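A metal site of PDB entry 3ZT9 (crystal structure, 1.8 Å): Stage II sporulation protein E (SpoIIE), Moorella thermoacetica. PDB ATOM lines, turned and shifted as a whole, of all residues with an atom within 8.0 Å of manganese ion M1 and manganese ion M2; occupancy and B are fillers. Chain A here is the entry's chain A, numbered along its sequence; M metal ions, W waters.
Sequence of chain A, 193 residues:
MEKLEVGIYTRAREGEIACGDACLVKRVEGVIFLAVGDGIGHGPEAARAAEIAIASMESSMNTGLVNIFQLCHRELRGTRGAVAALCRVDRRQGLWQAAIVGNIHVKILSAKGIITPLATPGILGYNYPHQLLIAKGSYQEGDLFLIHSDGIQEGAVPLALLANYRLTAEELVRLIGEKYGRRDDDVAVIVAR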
ATOM      1  N   CYS A  19       4.177  31.960  -3.687  1.00  0.00           N
ATOM      2  CA  CYS A  19       4.253  30.551  -3.306  1.00  0.00           C
ATOM      3  C   CYS A  19       5.608  30.205  -2.741  1.00  0.00           C
ATOM      4  O   CYS A  19       6.626  30.383  -3.389  1.00  0.00           O
ATOM      5  CB  CYS A  19       3.921  29.650  -4.503  1.00  0.00           C
ATOM      6  SG  CYS A  19       4.010  27.874  -4.188  1.00  0.00           S
ATOM      7  N   GLY A  20       5.623  29.669  -1.519  1.00  0.00           N
ATOM      8  CA  GLY A  20       6.896  29.314  -0.885  1.00  0.00           C
ATOM      9  C   GLY A  20       7.547  28.023  -1.335  1.00  0.00           C
ATOM     10  O   GLY A  20       8.612  27.684  -0.840  1.00  0.00           O
ATOM     11  N   ASP A  21       6.936  27.301  -2.272  1.00  0.00           N
ATOM     12  CA  ASP A  21       7.544  26.128  -2.883  1.00  0.00           C
ATOM     13  C   ASP A  21       8.036  26.491  -4.299  1.00  0.00           C
ATOM     14  O   ASP A  21       7.601  27.467  -4.894  1.00  0.00           O
ATOM     15  CB  ASP A  21       6.538  24.965  -3.038  1.00  0.00           C
ATOM     16  CG  ASP A  21       6.017  24.400  -1.728  1.00  0.00           C
ATOM     17  OD1 ASP A  21       6.565  24.672  -0.644  1.00  0.00           O
ATOM     18  OD2 ASP A  21       5.025  23.620  -1.817  1.00  0.00           O
ATOM     19  N   GLY A  37      11.340  22.212  -4.332  1.00  0.00           N
ATOM     20  CA  GLY A  37      11.870  22.747  -3.086  1.00  0.00           C
ATOM     21  C   GLY A  37      10.716  23.342  -2.288  1.00  0.00           C
ATOM     22  O   GLY A  37       9.712  23.795  -2.847  1.00  0.00           O
ATOM     23  N   ASP A  38      10.868  23.360  -0.969  1.00  0.00           N
ATOM     24  CA  ASP A  38       9.868  23.953  -0.107  1.00  0.00           C
ATOM     25  C   ASP A  38      10.624  24.835   0.863  1.00  0.00           C
ATOM     26  O   ASP A  38      11.324  24.320   1.714  1.00  0.00           O
ATOM     27  CB  ASP A  38       9.122  22.804   0.640  1.00  0.00           C
ATOM     28  CG  ASP A  38       8.139  23.302   1.698  1.00  0.00           C
ATOM     29  OD1 ASP A  38       8.175  24.502   2.033  1.00  0.00           O
ATOM     30  OD2 ASP A  38       7.345  22.478   2.220  1.00  0.00           O
ATOM     31  N   GLY A  39      10.527  26.158   0.727  1.00  0.00           N
ATOM     32  CA  GLY A  39      11.216  27.066   1.639  1.00  0.00           C
ATOM     33  C   GLY A  39      10.589  27.026   3.029  1.00  0.00           C
ATOM     34  O   GLY A  39       9.396  26.986   3.193  1.00  0.00           O
ATOM     35  N   ILE A  40      11.418  27.107   4.060  1.00  0.00           N
ATOM     36  CA  ILE A  40      10.866  26.969   5.403  1.00  0.00           C
ATOM     37  C   ILE A  40       9.804  28.046   5.606  1.00  0.00           C
ATOM     38  O   ILE A  40      10.045  29.235   5.340  1.00  0.00           O
ATOM     39  CB  ILE A  40      11.943  27.109   6.482  1.00  0.00           C
ATOM     40  CG1 ILE A  40      12.959  25.961   6.427  1.00  0.00           C
ATOM     41  CG2 ILE A  40      11.267  27.209   7.868  1.00  0.00           C
ATOM     42  CD1 ILE A  40      12.406  24.638   6.930  1.00  0.00           C
ATOM     43  N   GLY A  41       8.614  27.635   6.056  1.00  0.00           N
ATOM     44  CA  GLY A  41       7.556  28.592   6.350  1.00  0.00           C
ATOM     45  C   GLY A  41       6.814  28.888   5.070  1.00  0.00           C
ATOM     46  O   GLY A  41       6.774  28.061   4.155  1.00  0.00           O
ATOM     47  N   HIS A  42       6.244  30.074   4.990  1.00  0.00           N
ATOM     48  CA  HIS A  42       5.475  30.466   3.814  1.00  0.00           C
ATOM     49  C   HIS A  42       5.786  31.910   3.432  1.00  0.00           C
ATOM     50  O   HIS A  42       6.587  32.580   4.077  1.00  0.00           O
ATOM     51  CB  HIS A  42       3.963  30.271   4.031  1.00  0.00           C
ATOM     52  CG  HIS A  42       3.433  30.871   5.312  1.00  0.00           C
ATOM     53  ND1 HIS A  42       2.910  32.148   5.380  1.00  0.00           N
ATOM     54  CD2 HIS A  42       3.339  30.359   6.561  1.00  0.00           C
ATOM     55  CE1 HIS A  42       2.519  32.399   6.617  1.00  0.00           C
ATOM     56  NE2 HIS A  42       2.778  31.336   7.360  1.00  0.00           N
ATOM     57  N   GLY A  43       5.176  32.375   2.365  1.00  0.00           N
ATOM     58  CA  GLY A  43       5.303  33.770   1.983  1.00  0.00           C
ATOM     59  C   GLY A  43       6.568  34.056   1.179  1.00  0.00           C
ATOM     60  O   GLY A  43       7.292  33.144   0.803  1.00  0.00           O
ATOM     61  N   ALA A  46       9.974  32.478   2.232  1.00  0.00           N
ATOM     62  CA  ALA A  46      10.063  31.072   1.909  1.00  0.00           C
ATOM     63  C   ALA A  46      10.268  30.899   0.407  1.00  0.00           C
ATOM     64  O   ALA A  46      11.035  30.055   0.004  1.00  0.00           O
ATOM     65  CB  ALA A  46       8.804  30.321   2.362  1.00  0.00           C
ATOM     66  N   ALA A  47       9.565  31.706  -0.386  1.00  0.00           N
ATOM     67  CA  ALA A  47       9.671  31.621  -1.820  1.00  0.00           C
ATOM     68  C   ALA A  47      11.111  31.937  -2.262  1.00  0.00           C
ATOM     69  O   ALA A  47      11.675  31.275  -3.146  1.00  0.00           O
ATOM     70  CB  ALA A  47       8.670  32.620  -2.475  1.00  0.00           C
ATOM     71  N   ALA A  50      13.192  28.825  -1.626  1.00  0.00           N
ATOM     72  CA  ALA A  50      12.879  27.702  -2.525  1.00  0.00           C
ATOM     73  C   ALA A  50      13.441  28.001  -3.909  1.00  0.00           C
ATOM     74  O   ALA A  50      14.007  27.125  -4.553  1.00  0.00           O
ATOM     75  CB  ALA A  50      11.394  27.445  -2.606  1.00  0.00           C
ATOM     76  N   ARG A  80      15.745  31.613   4.805  1.00  0.00           N
ATOM     77  CA  ARG A  80      14.783  30.783   5.540  1.00  0.00           C
ATOM     78  C   ARG A  80      15.260  29.348   5.594  1.00  0.00           C
ATOM     79  O   ARG A  80      14.928  28.632   6.499  1.00  0.00           O
ATOM     80  CB  ARG A  80      13.384  30.803   4.901  1.00  0.00           C
ATOM     81  CG  ARG A  80      12.514  31.972   5.331  1.00  0.00           C
ATOM     82  CD  ARG A  80      11.848  31.723   6.707  1.00  0.00           C
ATOM     83  NE  ARG A  80      10.968  32.854   7.042  1.00  0.00           N
ATOM     84  CZ  ARG A  80       9.714  32.984   6.640  1.00  0.00           C
ATOM     85  NH1 ARG A  80       9.135  32.045   5.886  1.00  0.00           N
ATOM     86  NH2 ARG A  80       9.015  34.049   6.991  1.00  0.00           N
ATOM     87  N   GLY A  81      16.048  28.952   4.615  1.00  0.00           N
ATOM     88  CA  GLY A  81      16.406  27.540   4.438  1.00  0.00           C
ATOM     89  C   GLY A  81      15.328  26.841   3.627  1.00  0.00           C
ATOM     90  O   GLY A  81      14.256  27.375   3.428  1.00  0.00           O
ATOM     91  N   ALA A  82      15.595  25.629   3.161  1.00  0.00           N
ATOM     92  CA  ALA A  82      14.595  24.910   2.414  1.00  0.00           C
ATOM     93  C   ALA A  82      14.869  23.409   2.487  1.00  0.00           C
ATOM     94  O   ALA A  82      15.978  22.989   2.818  1.00  0.00           O
ATOM     95  CB  ALA A  82      14.664  25.352   0.945  1.00  0.00           C
ATOM     96  N   VAL A  83      13.847  22.613   2.193  1.00  0.00           N
ATOM     97  CA  VAL A  83      14.014  21.181   1.988  1.00  0.00           C
ATOM     98  C   VAL A  83      13.840  20.978   0.484  1.00  0.00           C
ATOM     99  O   VAL A  83      13.199  21.801  -0.160  1.00  0.00           O
ATOM    100  CB  VAL A  83      12.991  20.360   2.815  1.00  0.00           C
ATOM    101  CG1 VAL A  83      13.201  20.663   4.297  1.00  0.00           C
ATOM    102  CG2 VAL A  83      11.507  20.646   2.400  1.00  0.00           C
ATOM    103  N   ASN A 103      11.572  16.913   3.853  1.00  0.00           N
ATOM    104  CA  ASN A 103      10.365  16.083   3.713  1.00  0.00           C
ATOM    105  C   ASN A 103       9.613  16.263   2.400  1.00  0.00           C
ATOM    106  O   ASN A 103       8.421  16.178   2.354  1.00  0.00           O
ATOM    107  CB  ASN A 103       9.418  16.295   4.873  1.00  0.00           C
ATOM    108  CG  ASN A 103       8.797  17.675   4.845  1.00  0.00           C
ATOM    109  OD1 ASN A 103       9.293  18.575   4.162  1.00  0.00           O
ATOM    110  ND2 ASN A 103       7.693  17.851   5.580  1.00  0.00           N
ATOM    111  N   ILE A 104      10.316  16.495   1.313  1.00  0.00           N
ATOM    112  CA  ILE A 104       9.675  16.422   0.026  1.00  0.00           C
ATOM    113  C   ILE A 104       9.387  14.915  -0.258  1.00  0.00           C
ATOM    114  O   ILE A 104      10.137  14.032   0.162  1.00  0.00           O
ATOM    115  CB  ILE A 104      10.603  16.982  -1.077  1.00  0.00           C
ATOM    116  CG1 ILE A 104      10.973  18.451  -0.786  1.00  0.00           C
ATOM    117  CG2 ILE A 104       9.952  16.821  -2.450  1.00  0.00           C
ATOM    118  CD1 ILE A 104       9.815  19.458  -0.818  1.00  0.00           C
ATOM    119  N   SER A 149       5.675  18.542  -2.565  1.00  0.00           N
ATOM    120  CA  SER A 149       5.968  19.053  -1.217  1.00  0.00           C
ATOM    121  C   SER A 149       4.957  18.534  -0.217  1.00  0.00           C
ATOM    122  O   SER A 149       3.969  17.878  -0.596  1.00  0.00           O
ATOM    123  CB  SER A 149       5.879  20.576  -1.206  1.00  0.00           C
ATOM    124  OG  SER A 149       4.554  21.023  -1.453  1.00  0.00           O
ATOM    125  N   ASP A 150       5.193  18.815   1.067  1.00  0.00           N
ATOM    126  CA  ASP A 150       4.297  18.325   2.117  1.00  0.00           C
ATOM    127  C   ASP A 150       2.981  19.115   2.143  1.00  0.00           C
ATOM    128  O   ASP A 150       2.162  18.906   3.043  1.00  0.00           O
ATOM    129  CB  ASP A 150       5.016  18.377   3.466  1.00  0.00           C
ATOM    130  CG  ASP A 150       5.362  19.799   3.907  1.00  0.00           C
ATOM    131  OD1 ASP A 150       5.003  20.777   3.214  1.00  0.00           O
ATOM    132  OD2 ASP A 150       5.990  19.923   4.961  1.00  0.00           O
ATOM    133  N   GLY A 151       2.802  20.022   1.195  1.00  0.00           N
ATOM    134  CA  GLY A 151       1.463  20.542   0.881  1.00  0.00           C
ATOM    135  C   GLY A 151       0.489  19.442   0.497  1.00  0.00           C
ATOM    136  O   GLY A 151      -0.738  19.623   0.576  1.00  0.00           O
ATOM    137  N   ILE A 152       1.008  18.302   0.045  1.00  0.00           N
ATOM    138  CA  ILE A 152       0.193  17.083  -0.151  1.00  0.00           C
ATOM    139  C   ILE A 152       0.715  15.973   0.782  1.00  0.00           C
ATOM    140  O   ILE A 152       1.904  15.719   0.835  1.00  0.00           O
ATOM    141  CB  ILE A 152       0.212  16.596  -1.610  1.00  0.00           C
ATOM    142  CG1 ILE A 152      -0.456  17.637  -2.515  1.00  0.00           C
ATOM    143  CG2 ILE A 152      -0.501  15.227  -1.781  1.00  0.00           C
ATOM    144  CD1 ILE A 152      -0.250  17.393  -3.978  1.00  0.00           C
ATOM    145  N   ARG A 182      -3.276  20.854   0.540  1.00  0.00           N
ATOM    146  CA  ARG A 182      -3.810  21.587   1.687  1.00  0.00           C
ATOM    147  C   ARG A 182      -3.932  23.051   1.351  1.00  0.00           C
ATOM    148  O   ARG A 182      -3.085  23.596   0.663  1.00  0.00           O
ATOM    149  CB  ARG A 182      -2.880  21.459   2.894  1.00  0.00           C
ATOM    150  CG  ARG A 182      -2.633  20.038   3.331  1.00  0.00           C
ATOM    151  CD  ARG A 182      -1.630  20.036   4.457  1.00  0.00           C
ATOM    152  NE  ARG A 182      -2.170  20.741   5.606  1.00  0.00           N
ATOM    153  CZ  ARG A 182      -1.897  20.427   6.868  1.00  0.00           C
ATOM    154  NH1 ARG A 182      -1.081  19.422   7.145  1.00  0.00           N
ATOM    155  NH2 ARG A 182      -2.458  21.122   7.851  1.00  0.00           N
ATOM    156  N   ASP A 184      -3.821  25.357   3.700  1.00  0.00           N
ATOM    157  CA  ASP A 184      -3.034  26.053   4.712  1.00  0.00           C
ATOM    158  C   ASP A 184      -1.503  25.941   4.516  1.00  0.00           C
ATOM    159  O   ASP A 184      -0.718  26.377   5.353  1.00  0.00           O
ATOM    160  CB  ASP A 184      -3.460  25.640   6.141  1.00  0.00           C
ATOM    161  CG  ASP A 184      -3.075  24.207   6.485  1.00  0.00           C
ATOM    162  OD1 ASP A 184      -2.639  23.456   5.608  1.00  0.00           O
ATOM    163  OD2 ASP A 184      -3.222  23.797   7.652  1.00  0.00           O
ATOM    164  N   ASP A 185      -1.078  25.419   3.371  1.00  0.00           N
ATOM    165  CA  ASP A 185       0.347  25.405   3.083  1.00  0.00           C
ATOM    166  C   ASP A 185       0.476  25.588   1.598  1.00  0.00           C
ATOM    167  O   ASP A 185      -0.505  25.393   0.856  1.00  0.00           O
ATOM    168  CB  ASP A 185       1.005  24.079   3.522  1.00  0.00           C
ATOM    169  CG  ASP A 185       2.541  24.171   3.573  1.00  0.00           C
ATOM    170  OD1 ASP A 185       3.054  25.322   3.569  1.00  0.00           O
ATOM    171  OD2 ASP A 185       3.237  23.145   3.607  1.00  0.00           O
ATOM    172  N   ASP A 186       1.668  25.971   1.167  1.00  0.00           N
ATOM    173  CA  ASP A 186       2.009  25.961  -0.255  1.00  0.00           C
ATOM    174  C   ASP A 186       1.967  24.557  -0.804  1.00  0.00           C
ATOM    175  O   ASP A 186       2.237  23.614  -0.082  1.00  0.00           O
ATOM    176  CB  ASP A 186       3.407  26.507  -0.429  1.00  0.00           C
ATOM    177  CG  ASP A 186       3.534  27.928   0.106  1.00  0.00           C
ATOM    178  OD1 ASP A 186       2.848  28.801  -0.396  1.00  0.00           O
ATOM    179  OD2 ASP A 186       4.320  28.150   1.020  1.00  0.00           O
ATOM    180  N   VAL A 187       1.657  24.415  -2.094  1.00  0.00           N
ATOM    181  CA  VAL A 187       1.581  23.087  -2.724  1.00  0.00           C
ATOM    182  C   VAL A 187       2.449  23.105  -3.969  1.00  0.00           C
ATOM    183  O   VAL A 187       2.460  24.090  -4.722  1.00  0.00           O
ATOM    184  CB  VAL A 187       0.123  22.734  -3.071  1.00  0.00           C
ATOM    185  CG1 VAL A 187       0.045  21.503  -3.989  1.00  0.00           C
ATOM    186  CG2 VAL A 187      -0.712  22.524  -1.762  1.00  0.00           C
ATOM    187  N   ALA A 188       3.181  22.015  -4.215  1.00  0.00           N
ATOM    188  CA  ALA A 188       3.938  21.891  -5.441  1.00  0.00           C
ATOM    189  C   ALA A 188       3.923  20.429  -5.863  1.00  0.00           C
ATOM    190  O   ALA A 188       4.115  19.551  -5.027  1.00  0.00           O
ATOM    191  CB  ALA A 188       5.398  22.346  -5.231  1.00  0.00           C
HETATM  192 MN    MN M   1       7.390  26.120   3.210  1.00  0.00          MN
HETATM  193 MN    MN M   2       5.374  22.860   3.174  1.00  0.00          MN
HETATM  194  O   HOH W   1       5.609  24.966   3.869  1.00  0.00           O
HETATM  195  O   HOH W   2       7.863  24.917   5.119  1.00  0.00           O
HETATM  196  O   HOH W   3       6.490  26.623   1.289  1.00  0.00           O
HETATM  197  O   HOH W   4       4.720  23.429   1.150  1.00  0.00           O
HETATM  198  O   HOH W   5       6.148  22.759   5.266  1.00  0.00           O
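The backbone carbonyl oxygen (O) of Gly 20 lies within hydrogen-bond range of the backbone NH (N) of Gly 39, at 2.9 Å.
The backbone carbonyl oxygen (O) of Ile 40 lies within hydrogen-bond range of the guanidinium group (NH1) of Arg 80 (3.0 Å).
OD2 of Asp 150 is in hydrogen-bond range of ND2 of Asn 103 (2.8 Å).
The backbone carbonyl oxygen of Val 83 lies within hydrogen-bond range of the backbone NH of Asp 38, 2.9 Å away.
The backbone carbonyl oxygen (O) of Gly 81 lies within hydrogen-bond range of the backbone NH (N) of Ile 40 (2.9 Å).
Merely in contact with manganese ion M1: Ile 40 (3.9 Å).
Within 4 Å of manganese ion M1: Asp 38, Gly 39, Ile 40 and Gly 41.
The nearest printed residue that does not touch manganese ion M1 is Asp 21 (4.2 Å).
Of the 29 residues printed, 3 come within 4 Å of manganese ion M2.
Manganese ion M1 is bound by the side-chain carboxylate of Asp 38, water W3, the backbone carbonyl oxygen of Gly 39, water W1, the backbone carbonyl oxygen of Gly 41 and water W2.
Manganese ion M2 is bound by the side-chain carboxylate (OD1) of Asp 150 (2.1 Å), the side-chain carboxylate (OD2) of Asp 185 (2.2 Å), water W4 (2.2 Å), the side-chain carboxylate (OD2) of Asp 38 (2.2 Å), water W1 (2.2 Å) and water W5 (2.2 Å).
Manganese ion M2 has six donor atoms within binding distance.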
